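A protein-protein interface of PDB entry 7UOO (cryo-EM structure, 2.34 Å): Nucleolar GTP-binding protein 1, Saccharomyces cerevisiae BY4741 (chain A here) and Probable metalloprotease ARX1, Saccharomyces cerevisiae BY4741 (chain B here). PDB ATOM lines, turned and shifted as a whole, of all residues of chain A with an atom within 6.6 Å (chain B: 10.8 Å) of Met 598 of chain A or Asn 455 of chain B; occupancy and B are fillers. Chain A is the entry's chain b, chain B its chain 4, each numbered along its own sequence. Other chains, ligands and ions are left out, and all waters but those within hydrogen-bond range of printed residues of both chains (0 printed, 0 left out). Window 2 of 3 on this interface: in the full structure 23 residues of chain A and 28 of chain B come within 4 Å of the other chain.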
ATOM      1  N   VAL A 593      13.580  -2.484  35.365  1.00  0.00           N
ATOM      2  CA  VAL A 593      14.382  -2.261  34.165  1.00  0.00           C
ATOM      3  C   VAL A 593      15.728  -2.935  34.389  1.00  0.00           C
ATOM      4  O   VAL A 593      16.558  -2.443  35.163  1.00  0.00           O
ATOM      5  CB  VAL A 593      14.551  -0.768  33.852  1.00  0.00           C
ATOM      6  CG1 VAL A 593      15.365  -0.586  32.594  1.00  0.00           C
ATOM      7  CG2 VAL A 593      13.194  -0.092  33.707  1.00  0.00           C
ATOM      8  N   ALA A 594      15.950  -4.057  33.705  1.00  0.00           N
ATOM      9  CA  ALA A 594      17.091  -4.914  34.013  1.00  0.00           C
ATOM     10  C   ALA A 594      18.413  -4.344  33.507  1.00  0.00           C
ATOM     11  O   ALA A 594      19.432  -4.447  34.199  1.00  0.00           O
ATOM     12  CB  ALA A 594      16.865  -6.310  33.434  1.00  0.00           C
ATOM     13  N   ASP A 595      18.434  -3.748  32.318  1.00  0.00           N
ATOM     14  CA  ASP A 595      19.692  -3.369  31.692  1.00  0.00           C
ATOM     15  C   ASP A 595      19.921  -1.860  31.728  1.00  0.00           C
ATOM     16  O   ASP A 595      18.986  -1.053  31.644  1.00  0.00           O
ATOM     17  CB  ASP A 595      19.775  -3.887  30.252  1.00  0.00           C
ATOM     18  CG  ASP A 595      18.592  -3.487  29.414  1.00  0.00           C
ATOM     19  OD1 ASP A 595      17.469  -3.421  29.954  1.00  0.00           O
ATOM     20  OD2 ASP A 595      18.789  -3.246  28.206  1.00  0.00           O
ATOM     21  N   GLY A 596      21.201  -1.499  31.850  1.00  0.00           N
ATOM     22  CA  GLY A 596      21.568  -0.115  32.088  1.00  0.00           C
ATOM     23  C   GLY A 596      21.314   0.803  30.912  1.00  0.00           C
ATOM     24  O   GLY A 596      21.106   2.002  31.099  1.00  0.00           O
ATOM     25  N   SER A 597      21.329   0.265  29.692  1.00  0.00           N
ATOM     26  CA  SER A 597      21.003   1.078  28.526  1.00  0.00           C
ATOM     27  C   SER A 597      19.567   1.584  28.600  1.00  0.00           C
ATOM     28  O   SER A 597      19.301   2.780  28.419  1.00  0.00           O
ATOM     29  CB  SER A 597      21.231   0.269  27.250  1.00  0.00           C
ATOM     30  OG  SER A 597      20.948   1.040  26.097  1.00  0.00           O
ATOM     31  N   MET A 598      18.628   0.687  28.905  1.00  0.00           N
ATOM     32  CA  MET A 598      17.241   1.098  29.075  1.00  0.00           C
ATOM     33  C   MET A 598      17.059   1.952  30.322  1.00  0.00           C
ATOM     34  O   MET A 598      16.211   2.852  30.329  1.00  0.00           O
ATOM     35  CB  MET A 598      16.332  -0.128  29.123  1.00  0.00           C
ATOM     36  CG  MET A 598      16.464  -1.040  27.919  1.00  0.00           C
ATOM     37  SD  MET A 598      16.043  -0.243  26.359  1.00  0.00           S
ATOM     38  CE  MET A 598      14.259  -0.406  26.372  1.00  0.00           C
ATOM     39  N   ARG A 599      17.846   1.698  31.375  1.00  0.00           N
ATOM     40  CA  ARG A 599      17.801   2.568  32.548  1.00  0.00           C
ATOM     41  C   ARG A 599      18.184   4.000  32.190  1.00  0.00           C
ATOM     42  O   ARG A 599      17.520   4.957  32.605  1.00  0.00           O
ATOM     43  CB  ARG A 599      18.720   2.028  33.646  1.00  0.00           C
ATOM     44  CG  ARG A 599      18.151   0.848  34.398  1.00  0.00           C
ATOM     45  CD  ARG A 599      19.019   0.446  35.575  1.00  0.00           C
ATOM     46  NE  ARG A 599      18.378  -0.588  36.376  1.00  0.00           N
ATOM     47  CZ  ARG A 599      18.879  -1.091  37.496  1.00  0.00           C
ATOM     48  NH1 ARG A 599      20.039  -0.679  37.979  1.00  0.00           N
ATOM     49  NH2 ARG A 599      18.198  -2.028  38.148  1.00  0.00           N
ATOM     50  N   SER A 600      19.251   4.164  31.403  1.00  0.00           N
ATOM     51  CA  SER A 600      19.692   5.499  31.013  1.00  0.00           C
ATOM     52  C   SER A 600      18.703   6.150  30.054  1.00  0.00           C
ATOM     53  O   SER A 600      18.495   7.368  30.106  1.00  0.00           O
ATOM     54  CB  SER A 600      21.086   5.435  30.390  1.00  0.00           C
ATOM     55  OG  SER A 600      21.054   4.797  29.126  1.00  0.00           O
ATOM     56  N   LYS A 601      18.083   5.358  29.176  1.00  0.00           N
ATOM     57  CA  LYS A 601      17.048   5.908  28.305  1.00  0.00           C
ATOM     58  C   LYS A 601      15.856   6.420  29.108  1.00  0.00           C
ATOM     59  O   LYS A 601      15.334   7.508  28.835  1.00  0.00           O
ATOM     60  CB  LYS A 601      16.597   4.862  27.286  1.00  0.00           C
ATOM     61  CG  LYS A 601      15.538   5.379  26.335  1.00  0.00           C
ATOM     62  CD  LYS A 601      15.189   4.374  25.257  1.00  0.00           C
ATOM     63  CE  LYS A 601      14.378   3.228  25.809  1.00  0.00           C
ATOM     64  NZ  LYS A 601      13.713   2.479  24.712  1.00  0.00           N
ATOM     65  N   ALA A 602      15.417   5.652  30.109  1.00  0.00           N
ATOM     66  CA  ALA A 602      14.321   6.101  30.964  1.00  0.00           C
ATOM     67  C   ALA A 602      14.706   7.351  31.748  1.00  0.00           C
ATOM     68  O   ALA A 602      13.889   8.268  31.917  1.00  0.00           O
ATOM     69  CB  ALA A 602      13.903   4.977  31.911  1.00  0.00           C
ATOM     70  N   ASP A 603      15.950   7.402  32.233  1.00  0.00           N
ATOM     71  CA  ASP A 603      16.431   8.583  32.945  1.00  0.00           C
ATOM     72  C   ASP A 603      16.406   9.820  32.053  1.00  0.00           C
ATOM     73  O   ASP A 603      15.966  10.896  32.481  1.00  0.00           O
ATOM     74  CB  ASP A 603      17.842   8.323  33.471  1.00  0.00           C
ATOM     75  CG  ASP A 603      18.432   9.524  34.176  1.00  0.00           C
ATOM     76  OD1 ASP A 603      17.948   9.866  35.275  1.00  0.00           O
ATOM     77  OD2 ASP A 603      19.382  10.124  33.633  1.00  0.00           O
ATOM     78  N   ALA B 451      18.470 -13.925  16.055  1.00  0.00           N
ATOM     79  CA  ALA B 451      18.005 -13.056  17.123  1.00  0.00           C
ATOM     80  C   ALA B 451      18.302 -11.590  16.818  1.00  0.00           C
ATOM     81  O   ALA B 451      19.198 -11.253  16.039  1.00  0.00           O
ATOM     82  CB  ALA B 451      18.654 -13.446  18.445  1.00  0.00           C
ATOM     83  N   THR B 452      17.530 -10.713  17.454  1.00  0.00           N
ATOM     84  CA  THR B 452      17.688  -9.271  17.335  1.00  0.00           C
ATOM     85  C   THR B 452      17.940  -8.666  18.709  1.00  0.00           C
ATOM     86  O   THR B 452      17.279  -9.031  19.686  1.00  0.00           O
ATOM     87  CB  THR B 452      16.446  -8.623  16.716  1.00  0.00           C
ATOM     88  OG1 THR B 452      15.321  -8.825  17.580  1.00  0.00           O
ATOM     89  CG2 THR B 452      16.148  -9.227  15.351  1.00  0.00           C
ATOM     90  N   ASN B 453      18.896  -7.748  18.784  1.00  0.00           N
ATOM     91  CA  ASN B 453      19.143  -6.985  20.008  1.00  0.00           C
ATOM     92  C   ASN B 453      19.037  -5.498  19.705  1.00  0.00           C
ATOM     93  O   ASN B 453      19.908  -4.948  19.006  1.00  0.00           O
ATOM     94  CB  ASN B 453      20.508  -7.324  20.612  1.00  0.00           C
ATOM     95  CG  ASN B 453      21.613  -7.371  19.581  1.00  0.00           C
ATOM     96  OD1 ASN B 453      21.370  -7.634  18.404  1.00  0.00           O
ATOM     97  ND2 ASN B 453      22.839  -7.118  20.019  1.00  0.00           N
ATOM     98  N   PRO B 454      17.992  -4.814  20.178  1.00  0.00           N
ATOM     99  CA  PRO B 454      17.823  -3.391  19.837  1.00  0.00           C
ATOM    100  C   PRO B 454      18.904  -2.480  20.394  1.00  0.00           C
ATOM    101  O   PRO B 454      19.057  -1.362  19.890  1.00  0.00           O
ATOM    102  CB  PRO B 454      16.450  -3.048  20.433  1.00  0.00           C
ATOM    103  CG  PRO B 454      15.756  -4.361  20.581  1.00  0.00           C
ATOM    104  CD  PRO B 454      16.833  -5.345  20.912  1.00  0.00           C
ATOM    105  N   ASN B 455      19.653  -2.908  21.407  1.00  0.00           N
ATOM    106  CA  ASN B 455      20.664  -2.065  22.034  1.00  0.00           C
ATOM    107  C   ASN B 455      22.075  -2.338  21.532  1.00  0.00           C
ATOM    108  O   ASN B 455      22.874  -1.404  21.416  1.00  0.00           O
ATOM    109  CB  ASN B 455      20.619  -2.235  23.556  1.00  0.00           C
ATOM    110  CG  ASN B 455      19.370  -1.639  24.170  1.00  0.00           C
ATOM    111  OD1 ASN B 455      18.994  -0.507  23.863  1.00  0.00           O
ATOM    112  ND2 ASN B 455      18.716  -2.399  25.039  1.00  0.00           N
ATOM    113  N   GLY B 456      22.406  -3.591  21.229  1.00  0.00           N
ATOM    114  CA  GLY B 456      23.725  -3.920  20.723  1.00  0.00           C
ATOM    115  C   GLY B 456      24.816  -3.895  21.775  1.00  0.00           C
ATOM    116  O   GLY B 456      24.732  -4.603  22.783  1.00  0.00           O
ATOM    117  N   ASN B 457      25.848  -3.079  21.546  1.00  0.00           N
ATOM    118  CA  ASN B 457      26.964  -2.989  22.484  1.00  0.00           C
ATOM    119  C   ASN B 457      26.573  -2.310  23.790  1.00  0.00           C
ATOM    120  O   ASN B 457      27.215  -2.543  24.820  1.00  0.00           O
ATOM    121  CB  ASN B 457      28.125  -2.224  21.850  1.00  0.00           C
ATOM    122  CG  ASN B 457      28.922  -3.066  20.888  1.00  0.00           C
ATOM    123  OD1 ASN B 457      28.962  -4.290  21.003  1.00  0.00           O
ATOM    124  ND2 ASN B 457      29.574  -2.415  19.934  1.00  0.00           N
ATOM    125  N   LEU B 458      25.543  -1.463  23.766  1.00  0.00           N
ATOM    126  CA  LEU B 458      25.262  -0.600  24.909  1.00  0.00           C
ATOM    127  C   LEU B 458      24.705  -1.374  26.097  1.00  0.00           C
ATOM    128  O   LEU B 458      24.899  -0.962  27.245  1.00  0.00           O
ATOM    129  CB  LEU B 458      24.294   0.507  24.497  1.00  0.00           C
ATOM    130  CG  LEU B 458      24.763   1.427  23.369  1.00  0.00           C
ATOM    131  CD1 LEU B 458      23.612   2.270  22.857  1.00  0.00           C
ATOM    132  CD2 LEU B 458      25.907   2.311  23.835  1.00  0.00           C
ATOM    133  N   SER B 459      24.021  -2.487  25.849  1.00  0.00           N
ATOM    134  CA  SER B 459      23.335  -3.200  26.917  1.00  0.00           C
ATOM    135  C   SER B 459      24.320  -3.921  27.834  1.00  0.00           C
ATOM    136  O   SER B 459      25.379  -4.384  27.407  1.00  0.00           O
ATOM    137  CB  SER B 459      22.335  -4.196  26.331  1.00  0.00           C
ATOM    138  OG  SER B 459      22.966  -5.068  25.414  1.00  0.00           O
ATOM    139  N   TYR B 460      23.954  -4.001  29.111  1.00  0.00           N
ATOM    140  CA  TYR B 460      24.740  -4.692  30.125  1.00  0.00           C
ATOM    141  C   TYR B 460      23.842  -4.959  31.324  1.00  0.00           C
ATOM    142  O   TYR B 460      22.771  -4.365  31.459  1.00  0.00           O
ATOM    143  CB  TYR B 460      25.974  -3.880  30.540  1.00  0.00           C
ATOM    144  CG  TYR B 460      25.651  -2.575  31.238  1.00  0.00           C
ATOM    145  CD1 TYR B 460      25.402  -1.419  30.511  1.00  0.00           C
ATOM    146  CD2 TYR B 460      25.598  -2.499  32.625  1.00  0.00           C
ATOM    147  CE1 TYR B 460      25.104  -0.229  31.141  1.00  0.00           C
ATOM    148  CE2 TYR B 460      25.301  -1.313  33.265  1.00  0.00           C
ATOM    149  CZ  TYR B 460      25.057  -0.181  32.517  1.00  0.00           C
ATOM    150  OH  TYR B 460      24.761   1.005  33.147  1.00  0.00           O
ATOM    151  N   ASP B 461      24.302  -5.846  32.204  1.00  0.00           N
ATOM    152  CA  ASP B 461      23.558  -6.192  33.414  1.00  0.00           C
ATOM    153  C   ASP B 461      23.758  -5.103  34.461  1.00  0.00           C
ATOM    154  O   ASP B 461      24.869  -4.913  34.965  1.00  0.00           O
ATOM    155  CB  ASP B 461      24.013  -7.547  33.949  1.00  0.00           C
ATOM    156  CG  ASP B 461      23.445  -8.708  33.160  1.00  0.00           C
ATOM    157  OD1 ASP B 461      22.206  -8.854  33.128  1.00  0.00           O
ATOM    158  OD2 ASP B 461      24.239  -9.473  32.569  1.00  0.00           O
ATOM    159  N   ALA B 462      22.682  -4.393  34.802  1.00  0.00           N
ATOM    160  CA  ALA B 462      22.746  -3.352  35.818  1.00  0.00           C
ATOM    161  C   ALA B 462      22.406  -3.855  37.214  1.00  0.00           C
ATOM    162  O   ALA B 462      22.682  -3.151  38.193  1.00  0.00           O
ATOM    163  CB  ALA B 462      21.809  -2.196  35.455  1.00  0.00           C
ATOM    164  N   THR B 463      21.816  -5.041  37.333  1.00  0.00           N
ATOM    165  CA  THR B 463      21.523  -5.636  38.631  1.00  0.00           C
ATOM    166  C   THR B 463      22.608  -6.595  39.099  1.00  0.00           C
ATOM    167  O   THR B 463      22.471  -7.185  40.175  1.00  0.00           O
ATOM    168  CB  THR B 463      20.179  -6.373  38.591  1.00  0.00           C
ATOM    169  OG1 THR B 463      20.265  -7.480  37.688  1.00  0.00           O
ATOM    170  CG2 THR B 463      19.071  -5.440  38.135  1.00  0.00           C
ATOM    171  N   LEU B 473      31.270  -8.371  27.123  1.00  0.00           N
ATOM    172  CA  LEU B 473      30.917  -8.521  25.711  1.00  0.00           C
ATOM    173  C   LEU B 473      31.392  -9.890  25.246  1.00  0.00           C
ATOM    174  O   LEU B 473      32.513 -10.027  24.733  1.00  0.00           O
ATOM    175  CB  LEU B 473      31.528  -7.412  24.857  1.00  0.00           C
ATOM    176  CG  LEU B 473      30.742  -6.105  24.748  1.00  0.00           C
ATOM    177  CD1 LEU B 473      31.372  -5.186  23.715  1.00  0.00           C
ATOM    178  CD2 LEU B 473      29.285  -6.375  24.408  1.00  0.00           C
ATOM    179  N   LEU B 475      30.435 -11.534  22.683  1.00  0.00           N
ATOM    180  CA  LEU B 475      30.516 -11.528  21.221  1.00  0.00           C
ATOM    181  C   LEU B 475      30.733 -10.097  20.748  1.00  0.00           C
ATOM    182  O   LEU B 475      29.778  -9.408  20.364  1.00  0.00           O
ATOM    183  CB  LEU B 475      29.261 -12.136  20.595  1.00  0.00           C
ATOM    184  CG  LEU B 475      28.981 -13.600  20.940  1.00  0.00           C
ATOM    185  CD1 LEU B 475      27.654 -14.050  20.352  1.00  0.00           C
ATOM    186  CD2 LEU B 475      30.112 -14.488  20.455  1.00  0.00           C
ATOM    187  N   PRO B 476      31.978  -9.610  20.783  1.00  0.00           N
ATOM    188  CA  PRO B 476      32.234  -8.215  20.377  1.00  0.00           C
ATOM    189  C   PRO B 476      31.915  -7.921  18.921  1.00  0.00           C
ATOM    190  O   PRO B 476      31.432  -6.825  18.610  1.00  0.00           O
ATOM    191  CB  PRO B 476      33.732  -8.037  20.668  1.00  0.00           C
ATOM    192  CG  PRO B 476      34.091  -9.143  21.597  1.00  0.00           C
ATOM    193  CD  PRO B 476      33.206 -10.286  21.227  1.00  0.00           C
ATOM    194  N   LEU B 478      29.681  -9.432  16.836  1.00  0.00           N
ATOM    195  CA  LEU B 478      28.239  -9.378  16.647  1.00  0.00           C
ATOM    196  C   LEU B 478      27.567  -8.347  17.543  1.00  0.00           C
ATOM    197  O   LEU B 478      26.385  -8.051  17.339  1.00  0.00           O
ATOM    198  CB  LEU B 478      27.619 -10.754  16.900  1.00  0.00           C
ATOM    199  CG  LEU B 478      27.926 -11.846  15.873  1.00  0.00           C
ATOM    200  CD1 LEU B 478      27.585 -13.217  16.432  1.00  0.00           C
ATOM    201  CD2 LEU B 478      27.168 -11.590  14.583  1.00  0.00           C
ATOM    202  N   GLY B 479      28.285  -7.791  18.513  1.00  0.00           N
ATOM    203  CA  GLY B 479      27.700  -6.841  19.442  1.00  0.00           C
ATOM    204  C   GLY B 479      26.652  -7.434  20.359  1.00  0.00           C
ATOM    205  O   GLY B 479      25.607  -6.809  20.581  1.00  0.00           O
ATOM    206  N   VAL B 480      26.900  -8.625  20.893  1.00  0.00           N
ATOM    207  CA  VAL B 480      25.964  -9.313  21.775  1.00  0.00           C
ATOM    208  C   VAL B 480      26.545  -9.305  23.181  1.00  0.00           C
ATOM    209  O   VAL B 480      27.654  -9.803  23.406  1.00  0.00           O
ATOM    210  CB  VAL B 480      25.686 -10.748  21.301  1.00  0.00           C
ATOM    211  CG1 VAL B 480      24.665 -11.416  22.211  1.00  0.00           C
ATOM    212  CG2 VAL B 480      25.206 -10.749  19.860  1.00  0.00           C
ATOM    213  N   SER B 481      25.794  -8.748  24.124  1.00  0.00           N
ATOM    214  CA  SER B 481      26.226  -8.649  25.507  1.00  0.00           C
ATOM    215  C   SER B 481      25.892  -9.929  26.272  1.00  0.00           C
ATOM    216  O   SER B 481      25.244 -10.842  25.761  1.00  0.00           O
ATOM    217  CB  SER B 481      25.580  -7.439  26.178  1.00  0.00           C
ATOM    218  OG  SER B 481      24.167  -7.528  26.138  1.00  0.00           O
ATOM    219  N   ALA B 482      26.351  -9.984  27.526  1.00  0.00           N
ATOM    220  CA  ALA B 482      26.130 -11.167  28.353  1.00  0.00           C
ATOM    221  C   ALA B 482      24.659 -11.327  28.725  1.00  0.00           C
ATOM    222  O   ALA B 482      24.144 -12.450  28.765  1.00  0.00           O
ATOM    223  CB  ALA B 482      26.997 -11.098  29.609  1.00  0.00           C
ATOM    224  N   ILE B 483      23.970 -10.219  29.005  1.00  0.00           N
ATOM    225  CA  ILE B 483      22.546 -10.289  29.320  1.00  0.00           C
ATOM    226  C   ILE B 483      21.749 -10.754  28.103  1.00  0.00           C
ATOM    227  O   ILE B 483      20.845 -11.595  28.216  1.00  0.00           O
ATOM    228  CB  ILE B 483      22.055  -8.932  29.864  1.00  0.00           C
ATOM    229  CG1 ILE B 483      20.540  -8.938  30.078  1.00  0.00           C
ATOM    230  CG2 ILE B 483      22.498  -7.774  28.971  1.00  0.00           C
ATOM    231  CD1 ILE B 483      20.031  -7.738  30.843  1.00  0.00           C
ATOM    232  N   LYS B 484      22.099 -10.250  26.916  1.00  0.00           N
ATOM    233  CA  LYS B 484      21.452 -10.713  25.693  1.00  0.00           C
ATOM    234  C   LYS B 484      21.748 -12.185  25.437  1.00  0.00           C
ATOM    235  O   LYS B 484      20.870 -12.929  24.989  1.00  0.00           O
ATOM    236  CB  LYS B 484      21.893  -9.859  24.505  1.00  0.00           C
ATOM    237  CG  LYS B 484      21.131 -10.153  23.226  1.00  0.00           C
ATOM    238  CD  LYS B 484      19.632 -10.024  23.441  1.00  0.00           C
ATOM    239  CE  LYS B 484      18.857 -10.412  22.198  1.00  0.00           C
ATOM    240  NZ  LYS B 484      17.387 -10.390  22.431  1.00  0.00           N
ATOM    241  N   SER B 487      19.610 -14.241  27.641  1.00  0.00           N
ATOM    242  CA  SER B 487      18.270 -14.249  27.063  1.00  0.00           C
ATOM    243  C   SER B 487      18.168 -15.239  25.905  1.00  0.00           C
ATOM    244  O   SER B 487      17.183 -15.977  25.797  1.00  0.00           O
ATOM    245  CB  SER B 487      17.897 -12.841  26.603  1.00  0.00           C
ATOM    246  OG  SER B 487      16.602 -12.810  26.033  1.00  0.00           O
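The backbone carbonyl oxygen (O) of Ala 594 of chain A sits at hydrogen-bond distance from the backbone NH (N) of Ala 462 of chain B (3.3 Å). The side-chain carboxylate (OD2) of Asp 595 of chain A lies within hydrogen-bond range of the side-chain amide nitrogen (ND2) of Asn 455 of chain B (3.3 Å). The backbone NH of Gly 596 of chain A lies within hydrogen-bond range of the backbone carbonyl oxygen of Tyr 460 of chain B, at 3.3 Å. The side-chain amide oxygen (OD1) of Asn 455 of chain B sits at hydrogen-bond distance from the side-chain hydroxyl (OG) of Ser 597 of chain A. SD of Met 598 of chain A lies within hydrogen-bond range of ND2 of Asn 455 of chain B (3.7 Å).
NE of Arg 599 of chain A sits at hydrogen-bond distance from O of Val 593 of chain A (2.9 Å). The backbone carbonyl oxygen (O) of Gly 596 of chain A is in hydrogen-bond range of the side-chain hydroxyl (OG) of Ser 600 of chain A, at 3.4 Å. OG of Ser 600 of chain A sits at hydrogen-bond distance from O of Ser 597 of chain A (2.8 Å).
Among the printed residues, merely in contact across the chains: Ala 594 of chain A with Thr 463 of chain B (3.98 Å), Asp 595 of chain A with Tyr 460 of chain B (3.2 Å), Asp 595 of chain A with Ile 483 of chain B (3.9 Å), Gly 596 of chain A with Ala 462 of chain B (3.7 Å), Ser 597 of chain A with Leu 458 of chain B (3.7 Å), Arg 599 of chain A with Ala 462 of chain B (3.4 Å) and Arg 599 of chain A with Thr 463 of chain B (3.5 Å).
Of chain B, only Asn 455 (3.3 Å) and Leu 458 (3.7 Å) come within 4 Å of Ser 597 of chain A. Of chain B, only Asn 455 comes within 4 Å of Met 598 of chain A. Printed residues of chain B within 4 Å of Arg 599 of chain A: Ala 462 (3.4 Å) and Thr 463 (3.5 Å). No residue of chain B comes within 4 Å of Ser 600 of chain A. Lys 601 of chain A touches none of the printed residues of chain B. Of the printed residues of chain A, Asn 455 of chain B touches Asp 595 (3.3 Å), Ser 597 (3.3 Å) and Met 598 (3.7 Å). Printed residues of chain A within 4 Å of Leu 458 of chain B: Ser 597 (3.7 Å). Printed residues of chain A within 4 Å of Tyr 460 of chain B: Asp 595 and Gly 596. Of the printed residues of chain A, Thr 463 of chain B touches Ala 594 and Arg 599. The nearest residue of chain A that does not touch Asn 455 of chain B is Lys 601 of chain A (6.1 Å).
Of the 24 printed residues of chain B, 6 touch a printed residue of chain A. Hydrophobic or aromatic side chains of chain B within 4 Å of the printed part of chain A: Leu 458, Tyr 460, Ala 462 and Ile 483. Of the 11 printed residues of chain A, 6 touch a printed residue of chain B.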
